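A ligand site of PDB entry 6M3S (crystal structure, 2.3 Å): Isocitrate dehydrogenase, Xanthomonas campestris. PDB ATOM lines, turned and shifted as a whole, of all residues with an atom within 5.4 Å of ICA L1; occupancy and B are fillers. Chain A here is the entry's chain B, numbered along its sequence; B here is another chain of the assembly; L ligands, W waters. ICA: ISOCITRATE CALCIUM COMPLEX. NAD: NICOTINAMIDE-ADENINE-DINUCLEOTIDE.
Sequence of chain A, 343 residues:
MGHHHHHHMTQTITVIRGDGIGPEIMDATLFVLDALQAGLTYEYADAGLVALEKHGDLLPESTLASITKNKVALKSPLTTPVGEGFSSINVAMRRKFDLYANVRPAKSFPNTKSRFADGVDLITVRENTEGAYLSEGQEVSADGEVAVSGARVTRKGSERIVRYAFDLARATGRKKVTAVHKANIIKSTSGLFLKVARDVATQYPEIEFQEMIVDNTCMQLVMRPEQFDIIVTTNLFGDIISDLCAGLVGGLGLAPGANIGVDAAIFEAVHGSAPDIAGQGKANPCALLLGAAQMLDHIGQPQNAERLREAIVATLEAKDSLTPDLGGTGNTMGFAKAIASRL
A calcium atom (CA) of ICA L1 is bound by the side-chain carboxylate (OD1) of Asp 239 (2.3 Å). CA of ICA L1 is bound by OD2 of Asp 215 of chain B. The side-chain carboxylate of Asp 243 binds a calcium atom (CA) of ICA L1, at 2.5 Å. OG of Ser 88 is in hydrogen-bond range of O4 of ICA L1. An oxygen (O2) of ICA L1 is in salt-bridge range of the guanidinium group of Arg 94, 2.7 Å away. An oxygen (O5) of ICA L1 is in salt-bridge range of the guanidinium group of Arg 126. An oxygen (O6) of ICA L1 sits close to the side-chain hydroxyl (OH) of Tyr 133. An oxygen (O2) of ICA L1 is in salt-bridge range of the guanidinium group (NH2) of Arg 104 (3.3 Å). An oxygen (O4) of ICA L1 is in hydrogen-bond range of the side-chain amide nitrogen (ND2) of Asn 90, 3.2 Å away. NZ of Lys 182 of chain B lies within salt-bridge range of O6 of ICA L1 (3.4 Å). O3D of NAD L2 lies within hydrogen-bond range of N of Thr 80 (3.2 Å). An oxygen (O3D) of NAD L2 is in hydrogen-bond range of the backbone carbonyl oxygen of Thr 80 (2.7 Å). ND2 of Asn 90 is in hydrogen-bond range of O7N of NAD L2 (3.1 Å). An oxygen (O2D) of NAD L2 lies within hydrogen-bond range of the side-chain amide nitrogen (ND2) of Asn 184 of chain B (3.3 Å). An oxygen (O7N) of NAD L2 is in hydrogen-bond range of the backbone NH of Leu 78 (3.1 Å). OE2 of Glu 268 lies within hydrogen-bond range of N7N of NAD L2 (3.0 Å).
An oxygen (O2D) of NAD L2 sits at hydrogen-bond distance from an oxygen (O3) of ICA L1 (2.5 Å).
OD2 of Asp 239 is in hydrogen-bond range of OH of Tyr 133, at 3.0 Å. O of Asp 239 sits at hydrogen-bond distance from OG of Ser 242. OG of Ser 88 is in hydrogen-bond range of N of Asn 90, 3.2 Å away. NH2 of Arg 94 is in salt-bridge range of OE1 of Glu 268, at 3.1 Å. O of Asn 102 is in hydrogen-bond range of N of Arg 126, at 2.9 Å. OG of Ser 242 lies within hydrogen-bond range of NH1 of Arg 104 (3.0 Å). The side-chain amide nitrogen (ND2) of Asn 90 sits at hydrogen-bond distance from the backbone carbonyl oxygen (O) of Leu 78. The side-chain amide oxygen of Asn 184 of chain B lies close to the backbone carbonyl oxygen of Lys 182 of chain B.
The backbone carbonyl oxygen (O) of Val 270 lies close to an oxygen (O1) of ICA L1, at 3.4 Å. Thr 80 touches ICA L1 (CG2 to O3, 2.8 Å). Asn 184 of chain B touches ICA L1. Ile 185 of chain B touches ICA L1. Hydrophobic or aromatic side chains that line ICA L1: Tyr 133 and Ile 185 of chain B. The nearest printed residue that does not touch ICA L1 is Leu 78 (4.3 Å).
Water W2 bridges O of Val 270 and OD2 of Asp 243. Water W3 lies within hydrogen-bond range of ND2 of Asn 184 of chain B (3.0 Å) and NZ of Lys 182 of chain B (3.0 Å).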
ATOM      1  N   LEU A  78       9.643 -27.708 -24.533  1.00  0.00           N
ATOM      2  CA  LEU A  78       9.247 -27.608 -25.939  1.00  0.00           C
ATOM      3  C   LEU A  78       8.772 -26.187 -26.211  1.00  0.00           C
ATOM      4  O   LEU A  78       7.951 -25.673 -25.437  1.00  0.00           O
ATOM      5  CB  LEU A  78       8.099 -28.570 -26.202  1.00  0.00           C
ATOM      6  CG  LEU A  78       8.333 -30.003 -25.762  1.00  0.00           C
ATOM      7  CD1 LEU A  78       7.111 -30.844 -26.090  1.00  0.00           C
ATOM      8  CD2 LEU A  78       9.582 -30.582 -26.426  1.00  0.00           C
ATOM      9  N   THR A  79       9.242 -25.602 -27.297  1.00  0.00           N
ATOM     10  CA  THR A  79       8.771 -24.287 -27.765  1.00  0.00           C
ATOM     11  C   THR A  79       7.327 -24.442 -28.236  1.00  0.00           C
ATOM     12  O   THR A  79       7.033 -25.437 -28.907  1.00  0.00           O
ATOM     13  CB  THR A  79       9.675 -23.740 -28.872  1.00  0.00           C
ATOM     14  OG1 THR A  79      11.010 -23.802 -28.377  1.00  0.00           O
ATOM     15  CG2 THR A  79       9.333 -22.335 -29.303  1.00  0.00           C
ATOM     16  N   THR A  80       6.439 -23.513 -27.876  1.00  0.00           N
ATOM     17  CA  THR A  80       5.203 -23.325 -28.675  1.00  0.00           C
ATOM     18  C   THR A  80       5.177 -21.883 -29.138  1.00  0.00           C
ATOM     19  O   THR A  80       5.502 -20.969 -28.387  1.00  0.00           O
ATOM     20  CB  THR A  80       3.927 -23.886 -28.009  1.00  0.00           C
ATOM     21  OG1 THR A  80       2.818 -22.983 -28.114  1.00  0.00           O
ATOM     22  CG2 THR A  80       4.100 -24.313 -26.584  1.00  0.00           C
ATOM     23  N   SER A  88       0.195 -26.010 -28.271  1.00  0.00           N
ATOM     24  CA  SER A  88       1.184 -26.546 -27.302  1.00  0.00           C
ATOM     25  C   SER A  88       1.146 -28.069 -27.289  1.00  0.00           C
ATOM     26  O   SER A  88       0.062 -28.663 -27.076  1.00  0.00           O
ATOM     27  CB  SER A  88       0.936 -25.997 -25.921  1.00  0.00           C
ATOM     28  OG  SER A  88       1.737 -26.688 -24.991  1.00  0.00           O
ATOM     29  N   ASN A  90       3.075 -29.592 -24.999  1.00  0.00           N
ATOM     30  CA  ASN A  90       3.049 -29.786 -23.532  1.00  0.00           C
ATOM     31  C   ASN A  90       1.587 -30.049 -23.116  1.00  0.00           C
ATOM     32  O   ASN A  90       1.284 -31.107 -22.584  1.00  0.00           O
ATOM     33  CB  ASN A  90       3.683 -28.584 -22.833  1.00  0.00           C
ATOM     34  CG  ASN A  90       5.111 -28.369 -23.292  1.00  0.00           C
ATOM     35  OD1 ASN A  90       5.923 -29.278 -23.166  1.00  0.00           O
ATOM     36  ND2 ASN A  90       5.428 -27.214 -23.849  1.00  0.00           N
ATOM     37  N   VAL A  91       0.684 -29.129 -23.439  1.00  0.00           N
ATOM     38  CA  VAL A  91      -0.753 -29.302 -23.109  1.00  0.00           C
ATOM     39  C   VAL A  91      -1.293 -30.572 -23.791  1.00  0.00           C
ATOM     40  O   VAL A  91      -1.993 -31.345 -23.118  1.00  0.00           O
ATOM     41  CB  VAL A  91      -1.542 -28.058 -23.516  1.00  0.00           C
ATOM     42  CG1 VAL A  91      -3.048 -28.271 -23.366  1.00  0.00           C
ATOM     43  CG2 VAL A  91      -1.073 -26.855 -22.732  1.00  0.00           C
ATOM     44  N   ARG A  94      -0.245 -33.639 -21.914  1.00  0.00           N
ATOM     45  CA  ARG A  94      -0.933 -33.667 -20.595  1.00  0.00           C
ATOM     46  C   ARG A  94      -2.389 -34.124 -20.773  1.00  0.00           C
ATOM     47  O   ARG A  94      -2.862 -34.914 -19.967  1.00  0.00           O
ATOM     48  CB  ARG A  94      -0.896 -32.297 -19.914  1.00  0.00           C
ATOM     49  CG  ARG A  94       0.513 -31.839 -19.596  1.00  0.00           C
ATOM     50  CD  ARG A  94       0.499 -30.359 -19.324  1.00  0.00           C
ATOM     51  NE  ARG A  94       1.808 -29.901 -18.890  1.00  0.00           N
ATOM     52  CZ  ARG A  94       2.189 -28.636 -18.868  1.00  0.00           C
ATOM     53  NH1 ARG A  94       1.366 -27.679 -19.245  1.00  0.00           N
ATOM     54  NH2 ARG A  94       3.423 -28.341 -18.476  1.00  0.00           N
ATOM     55  N   ASN A 102      -0.360 -31.427 -11.846  1.00  0.00           N
ATOM     56  CA  ASN A 102       0.957 -30.800 -12.095  1.00  0.00           C
ATOM     57  C   ASN A 102       1.514 -30.365 -10.755  1.00  0.00           C
ATOM     58  O   ASN A 102       0.996 -29.394 -10.199  1.00  0.00           O
ATOM     59  CB  ASN A 102       0.845 -29.625 -13.037  1.00  0.00           C
ATOM     60  CG  ASN A 102       2.183 -29.204 -13.593  1.00  0.00           C
ATOM     61  OD1 ASN A 102       3.221 -29.335 -12.940  1.00  0.00           O
ATOM     62  ND2 ASN A 102       2.152 -28.643 -14.788  1.00  0.00           N
ATOM     63  N   ARG A 104       4.263 -28.902  -8.319  1.00  0.00           N
ATOM     64  CA  ARG A 104       5.387 -27.936  -8.412  1.00  0.00           C
ATOM     65  C   ARG A 104       5.836 -27.480  -7.035  1.00  0.00           C
ATOM     66  O   ARG A 104       5.359 -26.450  -6.539  1.00  0.00           O
ATOM     67  CB  ARG A 104       4.955 -26.766  -9.293  1.00  0.00           C
ATOM     68  CG  ARG A 104       4.642 -27.203 -10.721  1.00  0.00           C
ATOM     69  CD  ARG A 104       4.280 -26.146 -11.747  1.00  0.00           C
ATOM     70  NE  ARG A 104       4.325 -26.733 -13.070  1.00  0.00           N
ATOM     71  CZ  ARG A 104       4.394 -26.033 -14.201  1.00  0.00           C
ATOM     72  NH1 ARG A 104       4.333 -24.722 -14.172  1.00  0.00           N
ATOM     73  NH2 ARG A 104       4.490 -26.646 -15.355  1.00  0.00           N
ATOM     74  N   ARG A 126      -1.414 -27.925  -9.449  1.00  0.00           N
ATOM     75  CA  ARG A 126      -2.052 -27.162 -10.523  1.00  0.00           C
ATOM     76  C   ARG A 126      -2.881 -28.168 -11.311  1.00  0.00           C
ATOM     77  O   ARG A 126      -2.306 -29.191 -11.683  1.00  0.00           O
ATOM     78  CB  ARG A 126      -0.977 -26.455 -11.335  1.00  0.00           C
ATOM     79  CG  ARG A 126      -1.374 -26.113 -12.763  1.00  0.00           C
ATOM     80  CD  ARG A 126      -0.156 -25.789 -13.567  1.00  0.00           C
ATOM     81  NE  ARG A 126      -0.534 -25.320 -14.876  1.00  0.00           N
ATOM     82  CZ  ARG A 126       0.263 -25.171 -15.901  1.00  0.00           C
ATOM     83  NH1 ARG A 126       1.545 -25.461 -15.799  1.00  0.00           N
ATOM     84  NH2 ARG A 126      -0.235 -24.742 -17.040  1.00  0.00           N
ATOM     85  N   TYR A 133      -6.836 -23.426 -20.540  1.00  0.00           N
ATOM     86  CA  TYR A 133      -5.824 -23.942 -21.500  1.00  0.00           C
ATOM     87  C   TYR A 133      -6.519 -24.894 -22.469  1.00  0.00           C
ATOM     88  O   TYR A 133      -6.104 -26.048 -22.568  1.00  0.00           O
ATOM     89  CB  TYR A 133      -4.636 -24.573 -20.755  1.00  0.00           C
ATOM     90  CG  TYR A 133      -3.644 -23.571 -20.204  1.00  0.00           C
ATOM     91  CD1 TYR A 133      -3.961 -22.229 -20.163  1.00  0.00           C
ATOM     92  CD2 TYR A 133      -2.403 -23.962 -19.731  1.00  0.00           C
ATOM     93  CE1 TYR A 133      -3.070 -21.289 -19.671  1.00  0.00           C
ATOM     94  CE2 TYR A 133      -1.495 -23.020 -19.242  1.00  0.00           C
ATOM     95  CZ  TYR A 133      -1.836 -21.685 -19.203  1.00  0.00           C
ATOM     96  OH  TYR A 133      -0.993 -20.717 -18.730  1.00  0.00           O
ATOM     97  N   ASN A 235      -5.730 -24.426 -13.918  1.00  0.00           N
ATOM     98  CA  ASN A 235      -4.594 -24.626 -14.862  1.00  0.00           C
ATOM     99  C   ASN A 235      -3.795 -23.334 -15.067  1.00  0.00           C
ATOM    100  O   ASN A 235      -2.567 -23.349 -14.831  1.00  0.00           O
ATOM    101  CB  ASN A 235      -5.143 -25.208 -16.160  1.00  0.00           C
ATOM    102  CG  ASN A 235      -4.065 -25.847 -17.010  1.00  0.00           C
ATOM    103  OD1 ASN A 235      -2.886 -25.561 -16.823  1.00  0.00           O
ATOM    104  ND2 ASN A 235      -4.475 -26.714 -17.910  1.00  0.00           N
ATOM    105  N   ASP A 239      -0.248 -22.019 -13.330  1.00  0.00           N
ATOM    106  CA  ASP A 239       0.858 -21.615 -14.227  1.00  0.00           C
ATOM    107  C   ASP A 239       1.528 -20.333 -13.739  1.00  0.00           C
ATOM    108  O   ASP A 239       2.775 -20.315 -13.587  1.00  0.00           O
ATOM    109  CB  ASP A 239       0.372 -21.442 -15.657  1.00  0.00           C
ATOM    110  CG  ASP A 239       1.537 -21.322 -16.616  1.00  0.00           C
ATOM    111  OD1 ASP A 239       2.382 -22.266 -16.656  1.00  0.00           O
ATOM    112  OD2 ASP A 239       1.612 -20.264 -17.265  1.00  0.00           O
ATOM    113  N   SER A 242       3.097 -20.795  -9.973  1.00  0.00           N
ATOM    114  CA  SER A 242       4.311 -21.662  -9.861  1.00  0.00           C
ATOM    115  C   SER A 242       5.505 -20.930 -10.467  1.00  0.00           C
ATOM    116  O   SER A 242       6.622 -21.142  -9.961  1.00  0.00           O
ATOM    117  CB  SER A 242       4.113 -23.009 -10.479  1.00  0.00           C
ATOM    118  OG  SER A 242       3.938 -22.895 -11.874  1.00  0.00           O
ATOM    119  N   ASP A 243       5.302 -20.095 -11.497  1.00  0.00           N
ATOM    120  CA  ASP A 243       6.392 -19.240 -12.030  1.00  0.00           C
ATOM    121  C   ASP A 243       6.756 -18.158 -10.992  1.00  0.00           C
ATOM    122  O   ASP A 243       7.958 -17.966 -10.773  1.00  0.00           O
ATOM    123  CB  ASP A 243       6.040 -18.721 -13.411  1.00  0.00           C
ATOM    124  CG  ASP A 243       6.519 -19.587 -14.595  1.00  0.00           C
ATOM    125  OD1 ASP A 243       5.795 -20.663 -15.014  1.00  0.00           O
ATOM    126  OD2 ASP A 243       7.484 -19.100 -15.223  1.00  0.00           O
ATOM    127  N   GLU A 268       9.392 -32.908 -15.709  1.00  0.00           N
ATOM    128  CA  GLU A 268      10.068 -31.817 -16.422  1.00  0.00           C
ATOM    129  C   GLU A 268      10.382 -30.686 -15.453  1.00  0.00           C
ATOM    130  O   GLU A 268      10.019 -30.774 -14.254  1.00  0.00           O
ATOM    131  CB  GLU A 268       9.161 -31.351 -17.568  1.00  0.00           C
ATOM    132  CG  GLU A 268       7.821 -30.794 -17.145  1.00  0.00           C
ATOM    133  CD  GLU A 268       6.890 -30.339 -18.271  1.00  0.00           C
ATOM    134  OE1 GLU A 268       5.651 -30.391 -18.041  1.00  0.00           O
ATOM    135  OE2 GLU A 268       7.366 -29.909 -19.358  1.00  0.00           O
ATOM    136  N   VAL A 270       9.773 -26.518 -14.716  1.00  0.00           N
ATOM    137  CA  VAL A 270       8.699 -25.508 -14.880  1.00  0.00           C
ATOM    138  C   VAL A 270       9.059 -24.637 -16.089  1.00  0.00           C
ATOM    139  O   VAL A 270       8.141 -24.258 -16.805  1.00  0.00           O
ATOM    140  CB  VAL A 270       8.530 -24.686 -13.603  1.00  0.00           C
ATOM    141  CG1 VAL A 270       7.768 -23.405 -13.864  1.00  0.00           C
ATOM    142  CG2 VAL A 270       7.869 -25.529 -12.504  1.00  0.00           C
ATOM    143  N   LYS B 182      -0.448 -14.169 -23.001  1.00  0.00           N
ATOM    144  CA  LYS B 182      -0.266 -15.640 -23.041  1.00  0.00           C
ATOM    145  C   LYS B 182      -0.668 -16.107 -24.429  1.00  0.00           C
ATOM    146  O   LYS B 182      -1.405 -17.124 -24.571  1.00  0.00           O
ATOM    147  CB  LYS B 182      -1.048 -16.303 -21.895  1.00  0.00           C
ATOM    148  CG  LYS B 182      -0.736 -17.777 -21.667  1.00  0.00           C
ATOM    149  CD  LYS B 182       0.422 -18.012 -20.757  1.00  0.00           C
ATOM    150  CE  LYS B 182       0.888 -19.458 -20.765  1.00  0.00           C
ATOM    151  NZ  LYS B 182       2.027 -19.671 -19.851  1.00  0.00           N
ATOM    152  N   ASN B 184       0.851 -17.595 -26.658  1.00  0.00           N
ATOM    153  CA  ASN B 184       1.327 -18.952 -27.044  1.00  0.00           C
ATOM    154  C   ASN B 184       0.203 -19.989 -26.842  1.00  0.00           C
ATOM    155  O   ASN B 184       0.084 -20.910 -27.688  1.00  0.00           O
ATOM    156  CB  ASN B 184       2.600 -19.377 -26.302  1.00  0.00           C
ATOM    157  CG  ASN B 184       2.538 -19.222 -24.800  1.00  0.00           C
ATOM    158  OD1 ASN B 184       1.727 -18.451 -24.297  1.00  0.00           O
ATOM    159  ND2 ASN B 184       3.394 -19.923 -24.062  1.00  0.00           N
ATOM    160  N   ILE B 185      -0.589 -19.876 -25.776  1.00  0.00           N
ATOM    161  CA  ILE B 185      -1.651 -20.872 -25.436  1.00  0.00           C
ATOM    162  C   ILE B 185      -3.018 -20.343 -25.876  1.00  0.00           C
ATOM    163  O   ILE B 185      -3.813 -21.129 -26.397  1.00  0.00           O
ATOM    164  CB  ILE B 185      -1.644 -21.202 -23.933  1.00  0.00           C
ATOM    165  CG1 ILE B 185      -0.283 -21.737 -23.499  1.00  0.00           C
ATOM    166  CG2 ILE B 185      -2.768 -22.173 -23.594  1.00  0.00           C
ATOM    167  CD1 ILE B 185       0.125 -23.000 -24.211  1.00  0.00           C
ATOM    168  N   ASP B 215       3.558 -15.529 -17.121  1.00  0.00           N
ATOM    169  CA  ASP B 215       4.167 -16.357 -16.048  1.00  0.00           C
ATOM    170  C   ASP B 215       5.639 -15.939 -15.873  1.00  0.00           C
ATOM    171  O   ASP B 215       6.057 -15.703 -14.749  1.00  0.00           O
ATOM    172  CB  ASP B 215       3.995 -17.847 -16.338  1.00  0.00           C
ATOM    173  CG  ASP B 215       4.502 -18.254 -17.718  1.00  0.00           C
ATOM    174  OD1 ASP B 215       4.698 -17.349 -18.574  1.00  0.00           O
ATOM    175  OD2 ASP B 215       4.701 -19.482 -17.922  1.00  0.00           O
HETATM  176  C1  ICA L   1       4.167 -24.574 -18.302  1.00  0.00           C
HETATM  177  C2  ICA L   1       4.182 -23.640 -19.509  1.00  0.00           C
HETATM  178  C3  ICA L   1       3.255 -24.100 -20.625  1.00  0.00           C
HETATM  179  C4  ICA L   1       3.503 -23.276 -21.889  1.00  0.00           C
HETATM  180  C5  ICA L   1       3.660 -24.112 -23.142  1.00  0.00           C
HETATM  181  C6  ICA L   1       1.883 -23.947 -20.028  1.00  0.00           C
HETATM  182  O1  ICA L   1       4.799 -24.279 -17.231  1.00  0.00           O
HETATM  183  O2  ICA L   1       3.520 -25.644 -18.384  1.00  0.00           O
HETATM  184  O3  ICA L   1       4.470 -23.703 -23.924  1.00  0.00           O
HETATM  185  O4  ICA L   1       3.028 -25.131 -23.436  1.00  0.00           O
HETATM  186  O5  ICA L   1       1.550 -24.808 -19.187  1.00  0.00           O
HETATM  187  O6  ICA L   1       1.172 -22.951 -20.306  1.00  0.00           O
HETATM  188  O7  ICA L   1       3.948 -22.250 -19.117  1.00  0.00           O
HETATM  189 CA   ICA L   1       4.618 -21.643 -16.942  1.00  0.00          CA
HETATM  190  PA  NAD L   2      11.294 -19.328 -20.428  1.00  0.00           P
HETATM  191  O1A NAD L   2      11.735 -20.169 -21.554  1.00  0.00           O
HETATM  192  O2A NAD L   2      10.875 -20.207 -19.301  1.00  0.00           O
HETATM  193  O5B NAD L   2      12.400 -18.279 -19.960  1.00  0.00           O
HETATM  194  C5B NAD L   2      12.051 -17.113 -19.239  1.00  0.00           C
HETATM  195  C4B NAD L   2      13.345 -16.532 -18.680  1.00  0.00           C
HETATM  196  O4B NAD L   2      13.986 -17.398 -17.751  1.00  0.00           O
HETATM  197  C3B NAD L   2      14.343 -16.352 -19.805  1.00  0.00           C
HETATM  198  O3B NAD L   2      14.953 -15.091 -19.630  1.00  0.00           O
HETATM  199  C2B NAD L   2      15.301 -17.545 -19.688  1.00  0.00           C
HETATM  200  O2B NAD L   2      16.618 -17.332 -20.224  1.00  0.00           O
HETATM  201  C1B NAD L   2      15.278 -17.821 -18.192  1.00  0.00           C
HETATM  202  N9A NAD L   2      15.454 -19.244 -17.935  1.00  0.00           N
HETATM  203  C8A NAD L   2      14.533 -20.225 -18.118  1.00  0.00           C
HETATM  204  N7A NAD L   2      15.096 -21.402 -17.764  1.00  0.00           N
HETATM  205  C5A NAD L   2      16.352 -21.161 -17.405  1.00  0.00           C
HETATM  206  C6A NAD L   2      17.377 -21.967 -16.985  1.00  0.00           C
HETATM  207  N6A NAD L   2      17.182 -23.299 -16.859  1.00  0.00           N
HETATM  208  N1A NAD L   2      18.573 -21.395 -16.687  1.00  0.00           N
HETATM  209  C2A NAD L   2      18.750 -20.082 -16.795  1.00  0.00           C
HETATM  210  N3A NAD L   2      17.785 -19.283 -17.191  1.00  0.00           N
HETATM  211  C4A NAD L   2      16.573 -19.799 -17.501  1.00  0.00           C
HETATM  212  O3  NAD L   2       9.988 -18.486 -20.759  1.00  0.00           O
HETATM  213  PN  NAD L   2       9.517 -17.886 -22.135  1.00  0.00           P
HETATM  214  O1N NAD L   2       8.330 -17.086 -21.739  1.00  0.00           O
HETATM  215  O2N NAD L   2      10.530 -17.015 -22.819  1.00  0.00           O
HETATM  216  O5D NAD L   2       9.067 -19.075 -23.127  1.00  0.00           O
HETATM  217  C5D NAD L   2       9.835 -19.477 -24.258  1.00  0.00           C
HETATM  218  C4D NAD L   2       9.170 -20.720 -24.871  1.00  0.00           C
HETATM  219  O4D NAD L   2       9.139 -21.795 -23.913  1.00  0.00           O
HETATM  220  C3D NAD L   2       7.704 -20.460 -25.237  1.00  0.00           C
HETATM  221  O3D NAD L   2       7.559 -20.791 -26.601  1.00  0.00           O
HETATM  222  C2D NAD L   2       6.887 -21.372 -24.350  1.00  0.00           C
HETATM  223  O2D NAD L   2       5.803 -21.905 -25.070  1.00  0.00           O
HETATM  224  C1D NAD L   2       7.862 -22.446 -23.933  1.00  0.00           C
HETATM  225  N1N NAD L   2       7.601 -23.038 -22.616  1.00  0.00           N
HETATM  226  C2N NAD L   2       7.557 -24.363 -22.479  1.00  0.00           C
HETATM  227  C3N NAD L   2       7.349 -24.972 -21.261  1.00  0.00           C
HETATM  228  C7N NAD L   2       7.320 -26.475 -21.169  1.00  0.00           C
HETATM  229  O7N NAD L   2       7.907 -27.134 -22.023  1.00  0.00           O
HETATM  230  N7N NAD L   2       6.700 -27.082 -20.152  1.00  0.00           N
HETATM  231  C4N NAD L   2       7.203 -24.175 -20.111  1.00  0.00           C
HETATM  232  C5N NAD L   2       7.239 -22.777 -20.247  1.00  0.00           C
HETATM  233  C6N NAD L   2       7.447 -22.224 -21.523  1.00  0.00           C
HETATM  234  O   HOH W   1       6.435 -27.071 -17.484  1.00  0.00           O
HETATM  235  O   HOH W   2       7.249 -21.537 -17.268  1.00  0.00           O
HETATM  236  O   HOH W   3       4.641 -20.116 -21.335  1.00  0.00           O
